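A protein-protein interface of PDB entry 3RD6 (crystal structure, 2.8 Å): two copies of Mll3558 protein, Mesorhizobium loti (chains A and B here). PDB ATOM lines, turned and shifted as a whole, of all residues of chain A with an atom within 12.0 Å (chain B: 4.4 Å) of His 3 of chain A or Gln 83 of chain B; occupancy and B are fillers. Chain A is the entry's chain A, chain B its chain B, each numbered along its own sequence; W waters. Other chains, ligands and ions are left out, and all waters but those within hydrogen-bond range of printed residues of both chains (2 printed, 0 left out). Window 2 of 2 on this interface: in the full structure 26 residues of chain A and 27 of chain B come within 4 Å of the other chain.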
ATOM      1  N   HIS A   3     -11.130 -15.371   9.687  1.00  0.00           N
ATOM      2  CA  HIS A   3     -12.130 -15.727   8.635  1.00  0.00           C
ATOM      3  C   HIS A   3     -12.807 -17.079   8.891  1.00  0.00           C
ATOM      4  O   HIS A   3     -12.192 -18.005   9.425  1.00  0.00           O
ATOM      5  CB  HIS A   3     -11.457 -15.730   7.260  1.00  0.00           C
ATOM      6  CG  HIS A   3     -11.012 -14.374   6.810  1.00  0.00           C
ATOM      7  ND1 HIS A   3      -9.928 -13.722   7.364  1.00  0.00           N
ATOM      8  CD2 HIS A   3     -11.526 -13.535   5.884  1.00  0.00           C
ATOM      9  CE1 HIS A   3      -9.796 -12.539   6.792  1.00  0.00           C
ATOM     10  NE2 HIS A   3     -10.751 -12.398   5.890  1.00  0.00           N
ATOM     11  N   SER A   4     -14.073 -17.194   8.495  1.00  0.00           N
ATOM     12  CA  SER A   4     -14.821 -18.437   8.695  1.00  0.00           C
ATOM     13  C   SER A   4     -15.662 -18.832   7.491  1.00  0.00           C
ATOM     14  O   SER A   4     -16.131 -17.981   6.730  1.00  0.00           O
ATOM     15  CB  SER A   4     -15.738 -18.324   9.912  1.00  0.00           C
ATOM     16  OG  SER A   4     -15.003 -17.954  11.073  1.00  0.00           O
ATOM     17  N   VAL A   5     -15.861 -20.135   7.330  1.00  0.00           N
ATOM     18  CA  VAL A   5     -16.652 -20.638   6.219  1.00  0.00           C
ATOM     19  C   VAL A   5     -17.680 -21.635   6.707  1.00  0.00           C
ATOM     20  O   VAL A   5     -17.330 -22.650   7.300  1.00  0.00           O
ATOM     21  CB  VAL A   5     -15.780 -21.364   5.137  1.00  0.00           C
ATOM     22  CG1 VAL A   5     -16.663 -21.846   3.995  1.00  0.00           C
ATOM     23  CG2 VAL A   5     -14.703 -20.442   4.612  1.00  0.00           C
ATOM     24  N   ILE A   6     -18.950 -21.340   6.451  1.00  0.00           N
ATOM     25  CA  ILE A   6     -20.031 -22.240   6.833  1.00  0.00           C
ATOM     26  C   ILE A   6     -20.403 -23.050   5.586  1.00  0.00           C
ATOM     27  O   ILE A   6     -20.553 -22.487   4.496  1.00  0.00           O
ATOM     28  CB  ILE A   6     -21.283 -21.464   7.304  1.00  0.00           C
ATOM     29  CG1 ILE A   6     -20.964 -20.661   8.563  1.00  0.00           C
ATOM     30  CG2 ILE A   6     -22.425 -22.432   7.576  1.00  0.00           C
ATOM     31  CD1 ILE A   6     -22.155 -19.902   9.116  1.00  0.00           C
ATOM     32  N   HIS A   7     -20.523 -24.367   5.733  1.00  0.00           N
ATOM     33  CA  HIS A   7     -20.901 -25.221   4.616  1.00  0.00           C
ATOM     34  C   HIS A   7     -22.213 -25.873   4.949  1.00  0.00           C
ATOM     35  O   HIS A   7     -22.361 -26.457   6.016  1.00  0.00           O
ATOM     36  CB  HIS A   7     -19.885 -26.335   4.370  1.00  0.00           C
ATOM     37  CG  HIS A   7     -18.550 -25.846   3.913  1.00  0.00           C
ATOM     38  ND1 HIS A   7     -17.511 -25.599   4.782  1.00  0.00           N
ATOM     39  CD2 HIS A   7     -18.100 -25.510   2.685  1.00  0.00           C
ATOM     40  CE1 HIS A   7     -16.475 -25.132   4.111  1.00  0.00           C
ATOM     41  NE2 HIS A   7     -16.805 -25.068   2.834  1.00  0.00           N
ATOM     42  N   PRO A  95     -19.116  -4.482  -1.544  1.00  0.00           N
ATOM     43  CA  PRO A  95     -17.830  -5.123  -1.810  1.00  0.00           C
ATOM     44  C   PRO A  95     -17.625  -6.381  -0.957  1.00  0.00           C
ATOM     45  O   PRO A  95     -16.656  -7.124  -1.141  1.00  0.00           O
ATOM     46  CB  PRO A  95     -16.843  -4.023  -1.455  1.00  0.00           C
ATOM     47  CG  PRO A  95     -17.461  -3.488  -0.216  1.00  0.00           C
ATOM     48  CD  PRO A  95     -18.939  -3.380  -0.580  1.00  0.00           C
ATOM     49  N   GLN A  96     -18.537  -6.600  -0.013  1.00  0.00           N
ATOM     50  CA  GLN A  96     -18.460  -7.760   0.873  1.00  0.00           C
ATOM     51  C   GLN A  96     -19.010  -9.000   0.196  1.00  0.00           C
ATOM     52  O   GLN A  96     -20.197  -9.066  -0.101  1.00  0.00           O
ATOM     53  CB  GLN A  96     -19.260  -7.525   2.166  1.00  0.00           C
ATOM     54  CG  GLN A  96     -18.971  -6.195   2.855  1.00  0.00           C
ATOM     55  CD  GLN A  96     -17.596  -6.121   3.499  1.00  0.00           C
ATOM     56  OE1 GLN A  96     -16.987  -5.053   3.569  1.00  0.00           O
ATOM     57  NE2 GLN A  96     -17.108  -7.252   3.986  1.00  0.00           N
ATOM     58  N   PRO A  97     -18.147  -9.988  -0.093  1.00  0.00           N
ATOM     59  CA  PRO A  97     -18.572 -11.240  -0.737  1.00  0.00           C
ATOM     60  C   PRO A  97     -19.195 -12.155   0.302  1.00  0.00           C
ATOM     61  O   PRO A  97     -18.507 -12.668   1.177  1.00  0.00           O
ATOM     62  CB  PRO A  97     -17.270 -11.789  -1.308  1.00  0.00           C
ATOM     63  CG  PRO A  97     -16.261 -11.321  -0.331  1.00  0.00           C
ATOM     64  CD  PRO A  97     -16.676  -9.892  -0.072  1.00  0.00           C
ATOM     65  N   MET A  98     -20.504 -12.348   0.200  1.00  0.00           N
ATOM     66  CA  MET A  98     -21.216 -13.164   1.159  1.00  0.00           C
ATOM     67  C   MET A  98     -21.212 -14.679   0.974  1.00  0.00           C
ATOM     68  O   MET A  98     -21.427 -15.407   1.943  1.00  0.00           O
ATOM     69  CB  MET A  98     -22.662 -12.664   1.311  1.00  0.00           C
ATOM     70  CG  MET A  98     -23.371 -12.266   0.041  1.00  0.00           C
ATOM     71  SD  MET A  98     -24.933 -11.415   0.401  1.00  0.00           S
ATOM     72  CE  MET A  98     -25.942 -12.730   0.889  1.00  0.00           C
ATOM     73  N   SER A  99     -20.948 -15.175  -0.236  1.00  0.00           N
ATOM     74  CA  SER A  99     -20.944 -16.624  -0.444  1.00  0.00           C
ATOM     75  C   SER A  99     -20.680 -17.107  -1.855  1.00  0.00           C
ATOM     76  O   SER A  99     -20.774 -16.349  -2.805  1.00  0.00           O
ATOM     77  CB  SER A  99     -22.288 -17.180  -0.035  1.00  0.00           C
ATOM     78  OG  SER A  99     -23.263 -16.780  -0.987  1.00  0.00           O
ATOM     79  N   ALA A 123     -21.296 -22.243   0.414  1.00  0.00           N
ATOM     80  CA  ALA A 123     -20.230 -21.860   1.312  1.00  0.00           C
ATOM     81  C   ALA A 123     -20.498 -20.388   1.649  1.00  0.00           C
ATOM     82  O   ALA A 123     -20.341 -19.511   0.797  1.00  0.00           O
ATOM     83  CB  ALA A 123     -18.875 -22.029   0.609  1.00  0.00           C
ATOM     84  N   PHE A 124     -20.916 -20.129   2.886  1.00  0.00           N
ATOM     85  CA  PHE A 124     -21.227 -18.768   3.321  1.00  0.00           C
ATOM     86  C   PHE A 124     -20.038 -18.176   4.056  1.00  0.00           C
ATOM     87  O   PHE A 124     -19.501 -18.779   4.986  1.00  0.00           O
ATOM     88  CB  PHE A 124     -22.506 -18.782   4.169  1.00  0.00           C
ATOM     89  CG  PHE A 124     -23.627 -19.558   3.525  1.00  0.00           C
ATOM     90  CD1 PHE A 124     -23.666 -20.949   3.623  1.00  0.00           C
ATOM     91  CD2 PHE A 124     -24.579 -18.916   2.725  1.00  0.00           C
ATOM     92  CE1 PHE A 124     -24.627 -21.687   2.935  1.00  0.00           C
ATOM     93  CE2 PHE A 124     -25.543 -19.655   2.033  1.00  0.00           C
ATOM     94  CZ  PHE A 124     -25.561 -21.047   2.140  1.00  0.00           C
ATOM     95  N   PHE A 125     -19.658 -16.973   3.633  1.00  0.00           N
ATOM     96  CA  PHE A 125     -18.483 -16.297   4.151  1.00  0.00           C
ATOM     97  C   PHE A 125     -18.514 -15.378   5.349  1.00  0.00           C
ATOM     98  O   PHE A 125     -19.418 -14.572   5.539  1.00  0.00           O
ATOM     99  CB  PHE A 125     -17.780 -15.568   2.999  1.00  0.00           C
ATOM    100  CG  PHE A 125     -17.471 -16.465   1.831  1.00  0.00           C
ATOM    101  CD1 PHE A 125     -16.832 -17.686   2.024  1.00  0.00           C
ATOM    102  CD2 PHE A 125     -17.848 -16.112   0.547  1.00  0.00           C
ATOM    103  CE1 PHE A 125     -16.585 -18.528   0.958  1.00  0.00           C
ATOM    104  CE2 PHE A 125     -17.599 -16.957  -0.525  1.00  0.00           C
ATOM    105  CZ  PHE A 125     -16.968 -18.164  -0.316  1.00  0.00           C
ATOM    106  N   ASP A 126     -17.454 -15.537   6.133  1.00  0.00           N
ATOM    107  CA  ASP A 126     -17.156 -14.775   7.329  1.00  0.00           C
ATOM    108  C   ASP A 126     -18.330 -14.263   8.132  1.00  0.00           C
ATOM    109  O   ASP A 126     -18.880 -13.199   7.849  1.00  0.00           O
ATOM    110  CB  ASP A 126     -16.209 -13.630   6.954  1.00  0.00           C
ATOM    111  CG  ASP A 126     -14.935 -14.138   6.296  1.00  0.00           C
ATOM    112  OD1 ASP A 126     -14.400 -15.160   6.778  1.00  0.00           O
ATOM    113  OD2 ASP A 126     -14.466 -13.532   5.307  1.00  0.00           O
ATOM    114  N   GLY A 127     -18.683 -15.034   9.157  1.00  0.00           N
ATOM    115  CA  GLY A 127     -19.788 -14.685  10.028  1.00  0.00           C
ATOM    116  C   GLY A 127     -21.111 -14.956   9.352  1.00  0.00           C
ATOM    117  O   GLY A 127     -21.920 -15.754   9.825  1.00  0.00           O
ATOM    118  N   VAL A 128     -21.316 -14.282   8.227  1.00  0.00           N
ATOM    119  CA  VAL A 128     -22.537 -14.404   7.451  1.00  0.00           C
ATOM    120  C   VAL A 128     -23.065 -15.827   7.288  1.00  0.00           C
ATOM    121  O   VAL A 128     -22.365 -16.717   6.819  1.00  0.00           O
ATOM    122  CB  VAL A 128     -22.342 -13.774   6.041  1.00  0.00           C
ATOM    123  CG1 VAL A 128     -23.535 -14.081   5.144  1.00  0.00           C
ATOM    124  CG2 VAL A 128     -22.167 -12.278   6.176  1.00  0.00           C
ATOM    125  N   ASP A 129     -24.310 -16.029   7.709  1.00  0.00           N
ATOM    126  CA  ASP A 129     -24.977 -17.316   7.554  1.00  0.00           C
ATOM    127  C   ASP A 129     -26.295 -16.995   6.877  1.00  0.00           C
ATOM    128  O   ASP A 129     -27.320 -16.809   7.530  1.00  0.00           O
ATOM    129  CB  ASP A 129     -25.246 -18.009   8.894  1.00  0.00           C
ATOM    130  CG  ASP A 129     -25.832 -19.417   8.713  1.00  0.00           C
ATOM    131  OD1 ASP A 129     -26.874 -19.550   8.035  1.00  0.00           O
ATOM    132  OD2 ASP A 129     -25.251 -20.390   9.242  1.00  0.00           O
ATOM    133  N   PHE B  24      -0.327 -22.245   1.648  1.00  0.00           N
ATOM    134  CA  PHE B  24      -1.105 -21.470   0.686  1.00  0.00           C
ATOM    135  C   PHE B  24      -0.341 -21.325  -0.628  1.00  0.00           C
ATOM    136  O   PHE B  24      -0.941 -21.260  -1.706  1.00  0.00           O
ATOM    137  CB  PHE B  24      -1.402 -20.084   1.268  1.00  0.00           C
ATOM    138  CG  PHE B  24      -2.255 -19.222   0.384  1.00  0.00           C
ATOM    139  CD1 PHE B  24      -3.634 -19.398   0.338  1.00  0.00           C
ATOM    140  CD2 PHE B  24      -1.683 -18.219  -0.395  1.00  0.00           C
ATOM    141  CE1 PHE B  24      -4.430 -18.584  -0.468  1.00  0.00           C
ATOM    142  CE2 PHE B  24      -2.470 -17.404  -1.201  1.00  0.00           C
ATOM    143  CZ  PHE B  24      -3.843 -17.587  -1.235  1.00  0.00           C
ATOM    144  N   VAL B  80      -8.823 -15.586  -0.055  1.00  0.00           N
ATOM    145  CA  VAL B  80      -8.394 -14.874   1.163  1.00  0.00           C
ATOM    146  C   VAL B  80      -6.897 -15.134   1.363  1.00  0.00           C
ATOM    147  O   VAL B  80      -6.513 -16.181   1.906  1.00  0.00           O
ATOM    148  CB  VAL B  80      -9.139 -15.363   2.435  1.00  0.00           C
ATOM    149  CG1 VAL B  80      -8.660 -14.589   3.652  1.00  0.00           C
ATOM    150  CG2 VAL B  80     -10.643 -15.187   2.260  1.00  0.00           C
ATOM    151  N   PRO B  81      -6.036 -14.181   0.947  1.00  0.00           N
ATOM    152  CA  PRO B  81      -4.577 -14.304   1.067  1.00  0.00           C
ATOM    153  C   PRO B  81      -4.051 -15.066   2.281  1.00  0.00           C
ATOM    154  O   PRO B  81      -4.201 -14.632   3.422  1.00  0.00           O
ATOM    155  CB  PRO B  81      -4.114 -12.855   1.026  1.00  0.00           C
ATOM    156  CG  PRO B  81      -5.066 -12.255   0.027  1.00  0.00           C
ATOM    157  CD  PRO B  81      -6.400 -12.823   0.497  1.00  0.00           C
ATOM    158  N   ASP B  82      -3.442 -16.217   2.008  1.00  0.00           N
ATOM    159  CA  ASP B  82      -2.847 -17.085   3.030  1.00  0.00           C
ATOM    160  C   ASP B  82      -3.838 -17.732   3.993  1.00  0.00           C
ATOM    161  O   ASP B  82      -3.441 -18.350   4.984  1.00  0.00           O
ATOM    162  CB  ASP B  82      -1.796 -16.309   3.831  1.00  0.00           C
ATOM    163  CG  ASP B  82      -0.701 -15.731   2.948  1.00  0.00           C
ATOM    164  OD1 ASP B  82       0.013 -16.525   2.293  1.00  0.00           O
ATOM    165  OD2 ASP B  82      -0.557 -14.488   2.912  1.00  0.00           O
ATOM    166  N   GLN B  83      -5.126 -17.614   3.690  1.00  0.00           N
ATOM    167  CA  GLN B  83      -6.150 -18.187   4.552  1.00  0.00           C
ATOM    168  C   GLN B  83      -7.201 -19.048   3.848  1.00  0.00           C
ATOM    169  O   GLN B  83      -7.476 -20.192   4.262  1.00  0.00           O
ATOM    170  CB  GLN B  83      -6.859 -17.062   5.311  1.00  0.00           C
ATOM    171  CG  GLN B  83      -5.915 -16.085   6.019  1.00  0.00           C
ATOM    172  CD  GLN B  83      -6.653 -15.022   6.821  1.00  0.00           C
ATOM    173  OE1 GLN B  83      -7.466 -15.341   7.691  1.00  0.00           O
ATOM    174  NE2 GLN B  83      -6.369 -13.756   6.535  1.00  0.00           N
ATOM    175  N   ARG B  84      -7.785 -18.502   2.782  1.00  0.00           N
ATOM    176  CA  ARG B  84      -8.850 -19.207   2.080  1.00  0.00           C
ATOM    177  C   ARG B  84      -8.840 -19.206   0.562  1.00  0.00           C
ATOM    178  O   ARG B  84      -8.572 -18.193  -0.083  1.00  0.00           O
ATOM    179  CB  ARG B  84     -10.204 -18.664   2.559  1.00  0.00           C
ATOM    180  CG  ARG B  84     -11.398 -19.338   1.954  1.00  0.00           C
ATOM    181  CD  ARG B  84     -12.663 -18.928   2.653  1.00  0.00           C
ATOM    182  NE  ARG B  84     -13.017 -17.537   2.415  1.00  0.00           N
ATOM    183  CZ  ARG B  84     -13.589 -16.765   3.330  1.00  0.00           C
ATOM    184  NH1 ARG B  84     -13.853 -17.270   4.534  1.00  0.00           N
ATOM    185  NH2 ARG B  84     -13.903 -15.502   3.044  1.00  0.00           N
ATOM    186  N   VAL B 105     -10.791 -24.624   0.679  1.00  0.00           N
ATOM    187  CA  VAL B 105      -9.552 -25.046   1.302  1.00  0.00           C
ATOM    188  C   VAL B 105      -9.204 -23.927   2.278  1.00  0.00           C
ATOM    189  O   VAL B 105      -8.887 -22.795   1.879  1.00  0.00           O
ATOM    190  CB  VAL B 105      -8.399 -25.286   0.261  1.00  0.00           C
ATOM    191  CG1 VAL B 105      -8.310 -24.141  -0.710  1.00  0.00           C
ATOM    192  CG2 VAL B 105      -7.060 -25.454   0.982  1.00  0.00           C
ATOM    193  N   GLU B 106      -9.330 -24.235   3.564  1.00  0.00           N
ATOM    194  CA  GLU B 106      -9.018 -23.261   4.604  1.00  0.00           C
ATOM    195  C   GLU B 106      -7.803 -23.770   5.354  1.00  0.00           C
ATOM    196  O   GLU B 106      -7.609 -24.986   5.518  1.00  0.00           O
ATOM    197  CB  GLU B 106     -10.182 -23.095   5.587  1.00  0.00           C
ATOM    198  CG  GLU B 106     -11.468 -22.639   4.961  1.00  0.00           C
ATOM    199  CD  GLU B 106     -12.571 -22.534   5.979  1.00  0.00           C
ATOM    200  OE1 GLU B 106     -12.510 -21.610   6.824  1.00  0.00           O
ATOM    201  OE2 GLU B 106     -13.495 -23.378   5.938  1.00  0.00           O
ATOM    202  N   LEU B 107      -6.986 -22.840   5.821  1.00  0.00           N
ATOM    203  CA  LEU B 107      -5.789 -23.219   6.544  1.00  0.00           C
ATOM    204  C   LEU B 107      -5.522 -22.247   7.687  1.00  0.00           C
ATOM    205  O   LEU B 107      -4.887 -21.213   7.500  1.00  0.00           O
ATOM    206  CB  LEU B 107      -4.607 -23.290   5.563  1.00  0.00           C
ATOM    207  CG  LEU B 107      -4.736 -22.432   4.292  1.00  0.00           C
ATOM    208  CD1 LEU B 107      -4.581 -20.966   4.644  1.00  0.00           C
ATOM    209  CD2 LEU B 107      -3.680 -22.835   3.282  1.00  0.00           C
HETATM  210  O   HOH W   1     -14.313 -20.987   9.753  1.00  0.00           O
HETATM  211  O   HOH W   2     -14.768 -25.361   6.855  1.00  0.00           O
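Of chain B, only Val 80, Gln 83 and Arg 84 come within 4 Å of His 3 of chain A.
Of chain A, only His 3 (3.0 Å) comes within 4 Å of Gln 83 of chain B.
Pro 81 of chain B touches none of the printed residues of chain A.
Asp 82 of chain B touches none of the printed residues of chain A.
Of chain A, only His 3, Ser 4, Val 5, Phe 125 and Asp 126 come within 4 Å of Arg 84 of chain B.
No residue of chain A comes within 4 Å of Val 105 of chain B.
Glu 106 of chain B touches just these residues of chain A: Val 5 (3.1 Å) and His 7 (3.9 Å).
Printed residues of chain B within 4 Å of His 7 of chain A: Glu 106.
Printed residues of chain B within 4 Å of Phe 125 of chain A: Arg 84 (3.6 Å).
Printed residues of chain B within 4 Å of Val 5 of chain A: Arg 84 (3.2 Å) and Glu 106 (3.1 Å).
Of the printed residues of chain B, Asp 126 of chain A touches Arg 84.
Of the printed residues of chain B, Ser 4 of chain A touches Arg 84.
N of Ser 4 of chain A lies within hydrogen-bond range of OD1 of Asp 126 of chain A.
The backbone carbonyl oxygen (O) of Met 98 of chain A sits at hydrogen-bond distance from the backbone NH (N) of Phe 125 of chain A.
The backbone carbonyl oxygen (O) of Gln 83 of chain B lies close to the backbone NH (N) of Leu 107 of chain B (3.1 Å).
Water W2 lies within hydrogen-bond range of OE2 of Glu 106 of chain B (2.5 Å) and ND1 of His 7 of chain A (3.4 Å).
Water W1 lies within hydrogen-bond range of the backbone NH of Val 5 of chain A (3.0 Å), the side-chain hydroxyl of Ser 4 of chain A (3.4 Å) and the side-chain carboxylate of Glu 106 of chain B (3.5 Å).
Printed residues of chain A that touch a printed residue of chain B: His 3, Ser 4, Val 5, His 7, Phe 125 and Asp 126.
Hydrophobic or aromatic side chains of chain A within 4 Å of the printed part of chain B: His 3, Val 5, His 7 and Phe 125.
Of the 9 printed residues of chain B, 4 touch a printed residue of chain A.
Hydrophobic or aromatic side chains of chain B within 4 Å of the printed part of chain A: Val 80.
Among the printed residues, merely in contact across the chains: His 3 of chain A with Val 80 of chain B (3.8 Å), His 3 of chain A with Arg 84 of chain B (3.9 Å), Val 5 of chain A with Arg 84 of chain B (3.2 Å), Val 5 of chain A with Glu 106 of chain B (3.1 Å), His 7 of chain A with Glu 106 of chain B (3.9 Å) and Phe 125 of chain A with Arg 84 of chain B (3.6 Å).
No position is printed for both chains.
Of the 9 pairs that touch across the chains among the printed residues, none has its exchanged pair printed and touching as well.
A ring nitrogen (ND1) of His 3 of chain A lies within hydrogen-bond range of the side-chain amide oxygen (OE1) of Gln 83 of chain B (3.0 Å).
The backbone carbonyl oxygen (O) of Ser 4 of chain A sits at hydrogen-bond distance from the guanidinium group (NH1) of Arg 84 of chain B (3.2 Å).
The side-chain carboxylate of Asp 126 of chain A lies within salt-bridge range of the guanidinium group of Arg 84 of chain B.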
